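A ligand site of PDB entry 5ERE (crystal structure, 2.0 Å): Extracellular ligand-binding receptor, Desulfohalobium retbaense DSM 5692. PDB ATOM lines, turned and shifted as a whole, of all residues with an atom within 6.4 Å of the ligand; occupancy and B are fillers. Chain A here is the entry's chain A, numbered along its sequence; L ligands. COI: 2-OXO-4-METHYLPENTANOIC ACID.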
ATOM      1  N   PRO A   9      20.955 -18.993  11.860  1.00  0.00           N
ATOM      2  CA  PRO A   9      20.882 -20.426  11.558  1.00  0.00           C
ATOM      3  C   PRO A   9      21.139 -21.280  12.809  1.00  0.00           C
ATOM      4  O   PRO A   9      22.131 -22.001  12.854  1.00  0.00           O
ATOM      5  CB  PRO A   9      21.993 -20.595  10.511  1.00  0.00           C
ATOM      6  CG  PRO A   9      23.015 -19.504  10.899  1.00  0.00           C
ATOM      7  CD  PRO A   9      22.204 -18.382  11.376  1.00  0.00           C
ATOM      8  N   PHE A  14      26.081 -24.250  11.771  1.00  0.00           N
ATOM      9  CA  PHE A  14      26.617 -22.921  12.139  1.00  0.00           C
ATOM     10  C   PHE A  14      25.914 -22.348  13.375  1.00  0.00           C
ATOM     11  O   PHE A  14      25.841 -21.120  13.584  1.00  0.00           O
ATOM     12  CB  PHE A  14      26.519 -22.017  10.903  1.00  0.00           C
ATOM     13  CG  PHE A  14      27.034 -22.717   9.661  1.00  0.00           C
ATOM     14  CD1 PHE A  14      28.385 -23.029   9.563  1.00  0.00           C
ATOM     15  CD2 PHE A  14      26.171 -23.090   8.627  1.00  0.00           C
ATOM     16  CE1 PHE A  14      28.883 -23.705   8.434  1.00  0.00           C
ATOM     17  CE2 PHE A  14      26.670 -23.783   7.484  1.00  0.00           C
ATOM     18  CZ  PHE A  14      28.021 -24.066   7.392  1.00  0.00           C
ATOM     19  N   ILE A  17      27.951 -19.718  15.319  1.00  0.00           N
ATOM     20  CA  ILE A  17      27.927 -18.388  14.709  1.00  0.00           C
ATOM     21  C   ILE A  17      26.611 -17.706  15.063  1.00  0.00           C
ATOM     22  O   ILE A  17      26.582 -16.531  15.477  1.00  0.00           O
ATOM     23  CB  ILE A  17      28.125 -18.502  13.181  1.00  0.00           C
ATOM     24  CG1 ILE A  17      29.608 -18.807  12.888  1.00  0.00           C
ATOM     25  CG2 ILE A  17      27.654 -17.239  12.413  1.00  0.00           C
ATOM     26  CD1 ILE A  17      29.832 -19.448  11.529  1.00  0.00           C
ATOM     27  N   GLN A  21      26.059 -14.260  17.143  1.00  0.00           N
ATOM     28  CA  GLN A  21      25.327 -13.127  16.591  1.00  0.00           C
ATOM     29  C   GLN A  21      24.214 -12.697  17.559  1.00  0.00           C
ATOM     30  O   GLN A  21      24.007 -11.507  17.761  1.00  0.00           O
ATOM     31  CB  GLN A  21      24.763 -13.464  15.217  1.00  0.00           C
ATOM     32  CG  GLN A  21      25.827 -13.659  14.177  1.00  0.00           C
ATOM     33  CD  GLN A  21      25.276 -14.277  12.879  1.00  0.00           C
ATOM     34  OE1 GLN A  21      24.523 -15.241  12.914  1.00  0.00           O
ATOM     35  NE2 GLN A  21      25.629 -13.693  11.753  1.00  0.00           N
ATOM     36  N   CYS A  70      21.046 -13.893   8.604  1.00  0.00           N
ATOM     37  CA  CYS A  70      22.390 -14.434   8.507  1.00  0.00           C
ATOM     38  C   CYS A  70      22.442 -15.541   7.440  1.00  0.00           C
ATOM     39  O   CYS A  70      21.511 -16.308   7.344  1.00  0.00           O
ATOM     40  CB  CYS A  70      22.839 -14.998   9.855  1.00  0.00           C
ATOM     41  SG  CYS A  70      24.392 -15.931   9.646  1.00  0.00           S
ATOM     42  N   SER A  71      23.537 -15.553   6.679  1.00  0.00           N
ATOM     43  CA  SER A  71      23.997 -16.602   5.726  1.00  0.00           C
ATOM     44  C   SER A  71      23.679 -16.186   4.295  1.00  0.00           C
ATOM     45  O   SER A  71      22.654 -15.559   4.027  1.00  0.00           O
ATOM     46  CB  SER A  71      23.411 -17.993   6.017  1.00  0.00           C
ATOM     47  OG  SER A  71      22.116 -18.126   5.497  1.00  0.00           O
ATOM     48  N   SER A  72      24.605 -16.468   3.392  1.00  0.00           N
ATOM     49  CA  SER A  72      24.440 -16.147   1.973  1.00  0.00           C
ATOM     50  C   SER A  72      23.187 -16.782   1.379  1.00  0.00           C
ATOM     51  O   SER A  72      22.515 -16.161   0.558  1.00  0.00           O
ATOM     52  CB  SER A  72      25.669 -16.586   1.196  1.00  0.00           C
ATOM     53  OG  SER A  72      26.821 -15.942   1.717  1.00  0.00           O
ATOM     54  N   TRP A  73      22.840 -17.982   1.840  1.00  0.00           N
ATOM     55  CA  TRP A  73      21.667 -18.669   1.291  1.00  0.00           C
ATOM     56  C   TRP A  73      20.363 -18.116   1.835  1.00  0.00           C
ATOM     57  O   TRP A  73      19.430 -17.875   1.070  1.00  0.00           O
ATOM     58  CB  TRP A  73      21.735 -20.188   1.528  1.00  0.00           C
ATOM     59  CG  TRP A  73      22.149 -20.652   2.897  1.00  0.00           C
ATOM     60  CD1 TRP A  73      21.340 -21.136   3.884  1.00  0.00           C
ATOM     61  CD2 TRP A  73      23.489 -20.710   3.427  1.00  0.00           C
ATOM     62  NE1 TRP A  73      22.071 -21.468   4.981  1.00  0.00           N
ATOM     63  CE2 TRP A  73      23.398 -21.219   4.729  1.00  0.00           C
ATOM     64  CE3 TRP A  73      24.746 -20.365   2.914  1.00  0.00           C
ATOM     65  CZ2 TRP A  73      24.518 -21.404   5.533  1.00  0.00           C
ATOM     66  CZ3 TRP A  73      25.860 -20.543   3.715  1.00  0.00           C
ATOM     67  CH2 TRP A  73      25.729 -21.050   5.004  1.00  0.00           C
ATOM     68  N   ILE A  92      23.665 -10.080   6.935  1.00  0.00           N
ATOM     69  CA  ILE A  92      24.908 -10.206   7.675  1.00  0.00           C
ATOM     70  C   ILE A  92      25.432 -11.652   7.436  1.00  0.00           C
ATOM     71  O   ILE A  92      24.666 -12.527   6.975  1.00  0.00           O
ATOM     72  CB  ILE A  92      24.678  -9.914   9.161  1.00  0.00           C
ATOM     73  CG1 ILE A  92      23.667 -10.875   9.780  1.00  0.00           C
ATOM     74  CG2 ILE A  92      24.175  -8.434   9.322  1.00  0.00           C
ATOM     75  CD1 ILE A  92      23.665 -10.859  11.320  1.00  0.00           C
ATOM     76  N   GLY A  93      26.702 -11.892   7.711  1.00  0.00           N
ATOM     77  CA  GLY A  93      27.305 -13.206   7.411  1.00  0.00           C
ATOM     78  C   GLY A  93      26.893 -13.702   6.029  1.00  0.00           C
ATOM     79  O   GLY A  93      26.444 -14.846   5.847  1.00  0.00           O
ATOM     80  N   SER A  94      27.027 -12.837   5.039  1.00  0.00           N
ATOM     81  CA  SER A  94      26.466 -13.099   3.714  1.00  0.00           C
ATOM     82  C   SER A  94      27.387 -12.710   2.567  1.00  0.00           C
ATOM     83  O   SER A  94      27.013 -11.877   1.748  1.00  0.00           O
ATOM     84  CB  SER A  94      25.139 -12.350   3.537  1.00  0.00           C
ATOM     85  OG  SER A  94      24.099 -12.815   4.377  1.00  0.00           O
ATOM     86  N   ALA A  95      28.577 -13.308   2.457  1.00  0.00           N
ATOM     87  CA  ALA A  95      29.466 -12.943   1.323  1.00  0.00           C
ATOM     88  C   ALA A  95      28.942 -13.292  -0.105  1.00  0.00           C
ATOM     89  O   ALA A  95      29.379 -12.693  -1.083  1.00  0.00           O
ATOM     90  CB  ALA A  95      30.795 -13.568   1.494  1.00  0.00           C
ATOM     91  N   ALA A  96      28.055 -14.274  -0.250  1.00  0.00           N
ATOM     92  CA  ALA A  96      27.608 -14.669  -1.612  1.00  0.00           C
ATOM     93  C   ALA A  96      26.157 -14.242  -1.838  1.00  0.00           C
ATOM     94  O   ALA A  96      25.368 -14.969  -2.411  1.00  0.00           O
ATOM     95  CB  ALA A  96      27.777 -16.199  -1.856  1.00  0.00           C
ATOM     96  N   THR A 109      28.459  -7.625   4.872  1.00  0.00           N
ATOM     97  CA  THR A 109      29.555  -8.595   4.613  1.00  0.00           C
ATOM     98  C   THR A 109      30.219  -8.281   3.276  1.00  0.00           C
ATOM     99  O   THR A 109      29.544  -8.150   2.253  1.00  0.00           O
ATOM    100  CB  THR A 109      29.005 -10.040   4.582  1.00  0.00           C
ATOM    101  OG1 THR A 109      28.137 -10.251   5.709  1.00  0.00           O
ATOM    102  CG2 THR A 109      30.116 -11.094   4.519  1.00  0.00           C
ATOM    103  N   MET A 134      31.636 -26.101   1.447  1.00  0.00           N
ATOM    104  CA  MET A 134      30.290 -26.352   1.940  1.00  0.00           C
ATOM    105  C   MET A 134      29.329 -26.326   0.794  1.00  0.00           C
ATOM    106  O   MET A 134      29.428 -25.463  -0.074  1.00  0.00           O
ATOM    107  CB  MET A 134      29.895 -25.283   3.019  1.00  0.00           C
ATOM    108  CG  MET A 134      29.943 -23.870   2.542  1.00  0.00           C
ATOM    109  SD  MET A 134      29.433 -22.545   4.010  1.00  0.00           S
ATOM    110  CE  MET A 134      30.922 -22.806   5.237  1.00  0.00           C
ATOM    111  N   ASN A 136      26.521 -25.098  -0.445  1.00  0.00           N
ATOM    112  CA  ASN A 136      25.493 -24.086  -0.516  1.00  0.00           C
ATOM    113  C   ASN A 136      26.019 -22.971  -1.398  1.00  0.00           C
ATOM    114  O   ASN A 136      27.130 -23.087  -1.902  1.00  0.00           O
ATOM    115  CB  ASN A 136      25.117 -23.581   0.880  1.00  0.00           C
ATOM    116  CG  ASN A 136      26.330 -23.203   1.712  1.00  0.00           C
ATOM    117  OD1 ASN A 136      27.210 -22.479   1.262  1.00  0.00           O
ATOM    118  ND2 ASN A 136      26.372 -23.701   2.940  1.00  0.00           N
ATOM    119  N   ASN A 137      25.267 -21.883  -1.558  1.00  0.00           N
ATOM    120  CA  ASN A 137      25.681 -20.886  -2.526  1.00  0.00           C
ATOM    121  C   ASN A 137      26.991 -20.141  -2.119  1.00  0.00           C
ATOM    122  O   ASN A 137      27.650 -19.547  -2.969  1.00  0.00           O
ATOM    123  CB  ASN A 137      24.537 -19.883  -2.801  1.00  0.00           C
ATOM    124  CG  ASN A 137      24.219 -18.974  -1.583  1.00  0.00           C
ATOM    125  OD1 ASN A 137      24.428 -19.356  -0.446  1.00  0.00           O
ATOM    126  ND2 ASN A 137      23.671 -17.794  -1.842  1.00  0.00           N
ATOM    127  N   LEU A 138      27.398 -20.200  -0.847  1.00  0.00           N
ATOM    128  CA  LEU A 138      28.701 -19.641  -0.516  1.00  0.00           C
ATOM    129  C   LEU A 138      29.809 -20.543  -1.081  1.00  0.00           C
ATOM    130  O   LEU A 138      30.748 -20.063  -1.702  1.00  0.00           O
ATOM    131  CB  LEU A 138      28.886 -19.479   1.006  1.00  0.00           C
ATOM    132  CG  LEU A 138      30.253 -18.881   1.440  1.00  0.00           C
ATOM    133  CD1 LEU A 138      30.359 -17.383   1.136  1.00  0.00           C
ATOM    134  CD2 LEU A 138      30.531 -19.096   2.915  1.00  0.00           C
ATOM    135  N   SER A 186      34.830 -23.147   4.521  1.00  0.00           N
ATOM    136  CA  SER A 186      34.382 -23.731   5.764  1.00  0.00           C
ATOM    137  C   SER A 186      34.378 -22.700   6.889  1.00  0.00           C
ATOM    138  O   SER A 186      35.212 -21.783   6.944  1.00  0.00           O
ATOM    139  CB  SER A 186      35.292 -24.898   6.206  1.00  0.00           C
ATOM    140  OG  SER A 186      35.604 -25.780   5.158  1.00  0.00           O
ATOM    141  N   ALA A 187      33.461 -22.885   7.818  1.00  0.00           N
ATOM    142  CA  ALA A 187      33.551 -22.211   9.104  1.00  0.00           C
ATOM    143  C   ALA A 187      34.231 -23.184  10.086  1.00  0.00           C
ATOM    144  O   ALA A 187      35.239 -23.806   9.743  1.00  0.00           O
ATOM    145  CB  ALA A 187      32.147 -21.761   9.574  1.00  0.00           C
ATOM    146  N   ARG A 210      37.123 -15.933   5.490  1.00  0.00           N
ATOM    147  CA  ARG A 210      36.646 -15.215   6.684  1.00  0.00           C
ATOM    148  C   ARG A 210      35.984 -16.072   7.777  1.00  0.00           C
ATOM    149  O   ARG A 210      36.349 -15.974   8.938  1.00  0.00           O
ATOM    150  CB  ARG A 210      35.679 -14.084   6.209  1.00  0.00           C
ATOM    151  CG  ARG A 210      34.828 -13.438   7.324  1.00  0.00           C
ATOM    152  CD  ARG A 210      33.740 -12.480   6.666  1.00  0.00           C
ATOM    153  NE  ARG A 210      33.107 -13.185   5.562  1.00  0.00           N
ATOM    154  CZ  ARG A 210      32.055 -13.980   5.657  1.00  0.00           C
ATOM    155  NH1 ARG A 210      31.455 -14.162   6.815  1.00  0.00           N
ATOM    156  NH2 ARG A 210      31.607 -14.634   4.584  1.00  0.00           N
ATOM    157  N   PRO A 211      35.016 -16.933   7.434  1.00  0.00           N
ATOM    158  CA  PRO A 211      34.295 -17.776   8.401  1.00  0.00           C
ATOM    159  C   PRO A 211      35.147 -18.750   9.218  1.00  0.00           C
ATOM    160  O   PRO A 211      34.678 -19.232  10.255  1.00  0.00           O
ATOM    161  CB  PRO A 211      33.345 -18.582   7.500  1.00  0.00           C
ATOM    162  CG  PRO A 211      33.190 -17.744   6.300  1.00  0.00           C
ATOM    163  CD  PRO A 211      34.536 -17.181   6.061  1.00  0.00           C
ATOM    164  N   PHE A 254      34.132 -12.629  13.879  1.00  0.00           N
ATOM    165  CA  PHE A 254      33.643 -11.705  12.866  1.00  0.00           C
ATOM    166  C   PHE A 254      32.157 -11.455  12.974  1.00  0.00           C
ATOM    167  O   PHE A 254      31.679 -10.315  12.816  1.00  0.00           O
ATOM    168  CB  PHE A 254      33.921 -12.225  11.438  1.00  0.00           C
ATOM    169  CG  PHE A 254      33.100 -11.530  10.420  1.00  0.00           C
ATOM    170  CD1 PHE A 254      33.469 -10.275   9.978  1.00  0.00           C
ATOM    171  CD2 PHE A 254      31.919 -12.081   9.958  1.00  0.00           C
ATOM    172  CE1 PHE A 254      32.680  -9.577   9.083  1.00  0.00           C
ATOM    173  CE2 PHE A 254      31.123 -11.387   9.069  1.00  0.00           C
ATOM    174  CZ  PHE A 254      31.508 -10.130   8.633  1.00  0.00           C
ATOM    175  N   PHE A 255      31.414 -12.525  13.196  1.00  0.00           N
ATOM    176  CA  PHE A 255      29.967 -12.395  13.098  1.00  0.00           C
ATOM    177  C   PHE A 255      29.382 -11.573  14.235  1.00  0.00           C
ATOM    178  O   PHE A 255      28.465 -10.810  14.004  1.00  0.00           O
ATOM    179  CB  PHE A 255      29.335 -13.765  13.058  1.00  0.00           C
ATOM    180  CG  PHE A 255      29.805 -14.587  11.896  1.00  0.00           C
ATOM    181  CD1 PHE A 255      29.161 -14.511  10.676  1.00  0.00           C
ATOM    182  CD2 PHE A 255      30.912 -15.439  12.024  1.00  0.00           C
ATOM    183  CE1 PHE A 255      29.590 -15.268   9.572  1.00  0.00           C
ATOM    184  CE2 PHE A 255      31.354 -16.198  10.917  1.00  0.00           C
ATOM    185  CZ  PHE A 255      30.684 -16.105   9.695  1.00  0.00           C
HETATM  186  C1  COI L   1      28.368 -16.510   4.438  1.00  0.00           C
HETATM  187  O1  COI L   1      27.371 -17.001   3.842  1.00  0.00           O
HETATM  188  O2  COI L   1      29.081 -15.610   3.928  1.00  0.00           O
HETATM  189  C2  COI L   1      28.656 -16.967   5.830  1.00  0.00           C
HETATM  190  O3  COI L   1      29.627 -16.541   6.427  1.00  0.00           O
HETATM  191  C3  COI L   1      27.659 -17.941   6.417  1.00  0.00           C
HETATM  192  C4  COI L   1      28.159 -18.461   7.721  1.00  0.00           C
HETATM  193  C5  COI L   1      26.946 -18.903   8.515  1.00  0.00           C
HETATM  194  C6  COI L   1      29.110 -19.596   7.367  1.00  0.00           C
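Merely in contact with the ligand: Phe 14 (3.9 Å), Ser 71 (3.8 Å), Trp 73 (3.9 Å), Ser 94 (3.6 Å), Leu 138 (3.5 Å), Pro 211 (3.8 Å) and Phe 255 (3.4 Å). Hydrophobic or aromatic side chains that line the ligand: Phe 14, Trp 73, Ala 95, Leu 138, Pro 211 and Phe 255. Within 4 Å of the ligand: Phe 14, Ser 71, Ser 72, Trp 73, Gly 93, Ser 94, Ala 95, Leu 138, Arg 210, Pro 211 and Phe 255. The nearest printed residue that does not touch the ligand is Cys 70 (4.1 Å).
An oxygen (O1) of the ligand is in hydrogen-bond range of the backbone NH of Ser 72 (2.9 Å). OG of Ser 72 lies within hydrogen-bond range of O1 of the ligand (2.4 Å). The backbone NH (N) of Ala 95 is in hydrogen-bond range of an oxygen (O2) of the ligand. An oxygen (O2) of the ligand lies within salt-bridge range of the guanidinium group (NH2) of Arg 210, 2.8 Å away. The backbone carbonyl oxygen (O) of Gly 93 lies close to an oxygen (O1) of the ligand, at 3.1 Å.
O of Gly 93 is in hydrogen-bond range of N of Ser 72, 3.5 Å away. The backbone carbonyl oxygen of Ser 72 lies within hydrogen-bond range of the side-chain amide nitrogen of Asn 137 (3.1 Å). The backbone NH (N) of Ser 71 lies close to the backbone carbonyl oxygen (O) of Gly 93 (3.1 Å). The side-chain hydroxyl (OG) of Ser 94 sits at hydrogen-bond distance from the backbone carbonyl oxygen (O) of Ser 71 (3.1 Å). The backbone NH (N) of Ser 94 is in hydrogen-bond range of the side-chain hydroxyl (OG1) of Thr 109, 2.9 Å away. The side-chain hydroxyl (OG) of Ser 94 is in hydrogen-bond range of the backbone carbonyl oxygen (O) of Ile 92, at 2.7 Å. The indole nitrogen (NE1) of Trp 73 lies within hydrogen-bond range of the side-chain hydroxyl (OG) of Ser 71. N of Ser 71 lies within hydrogen-bond range of O of Ile 92, 3.2 Å away.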
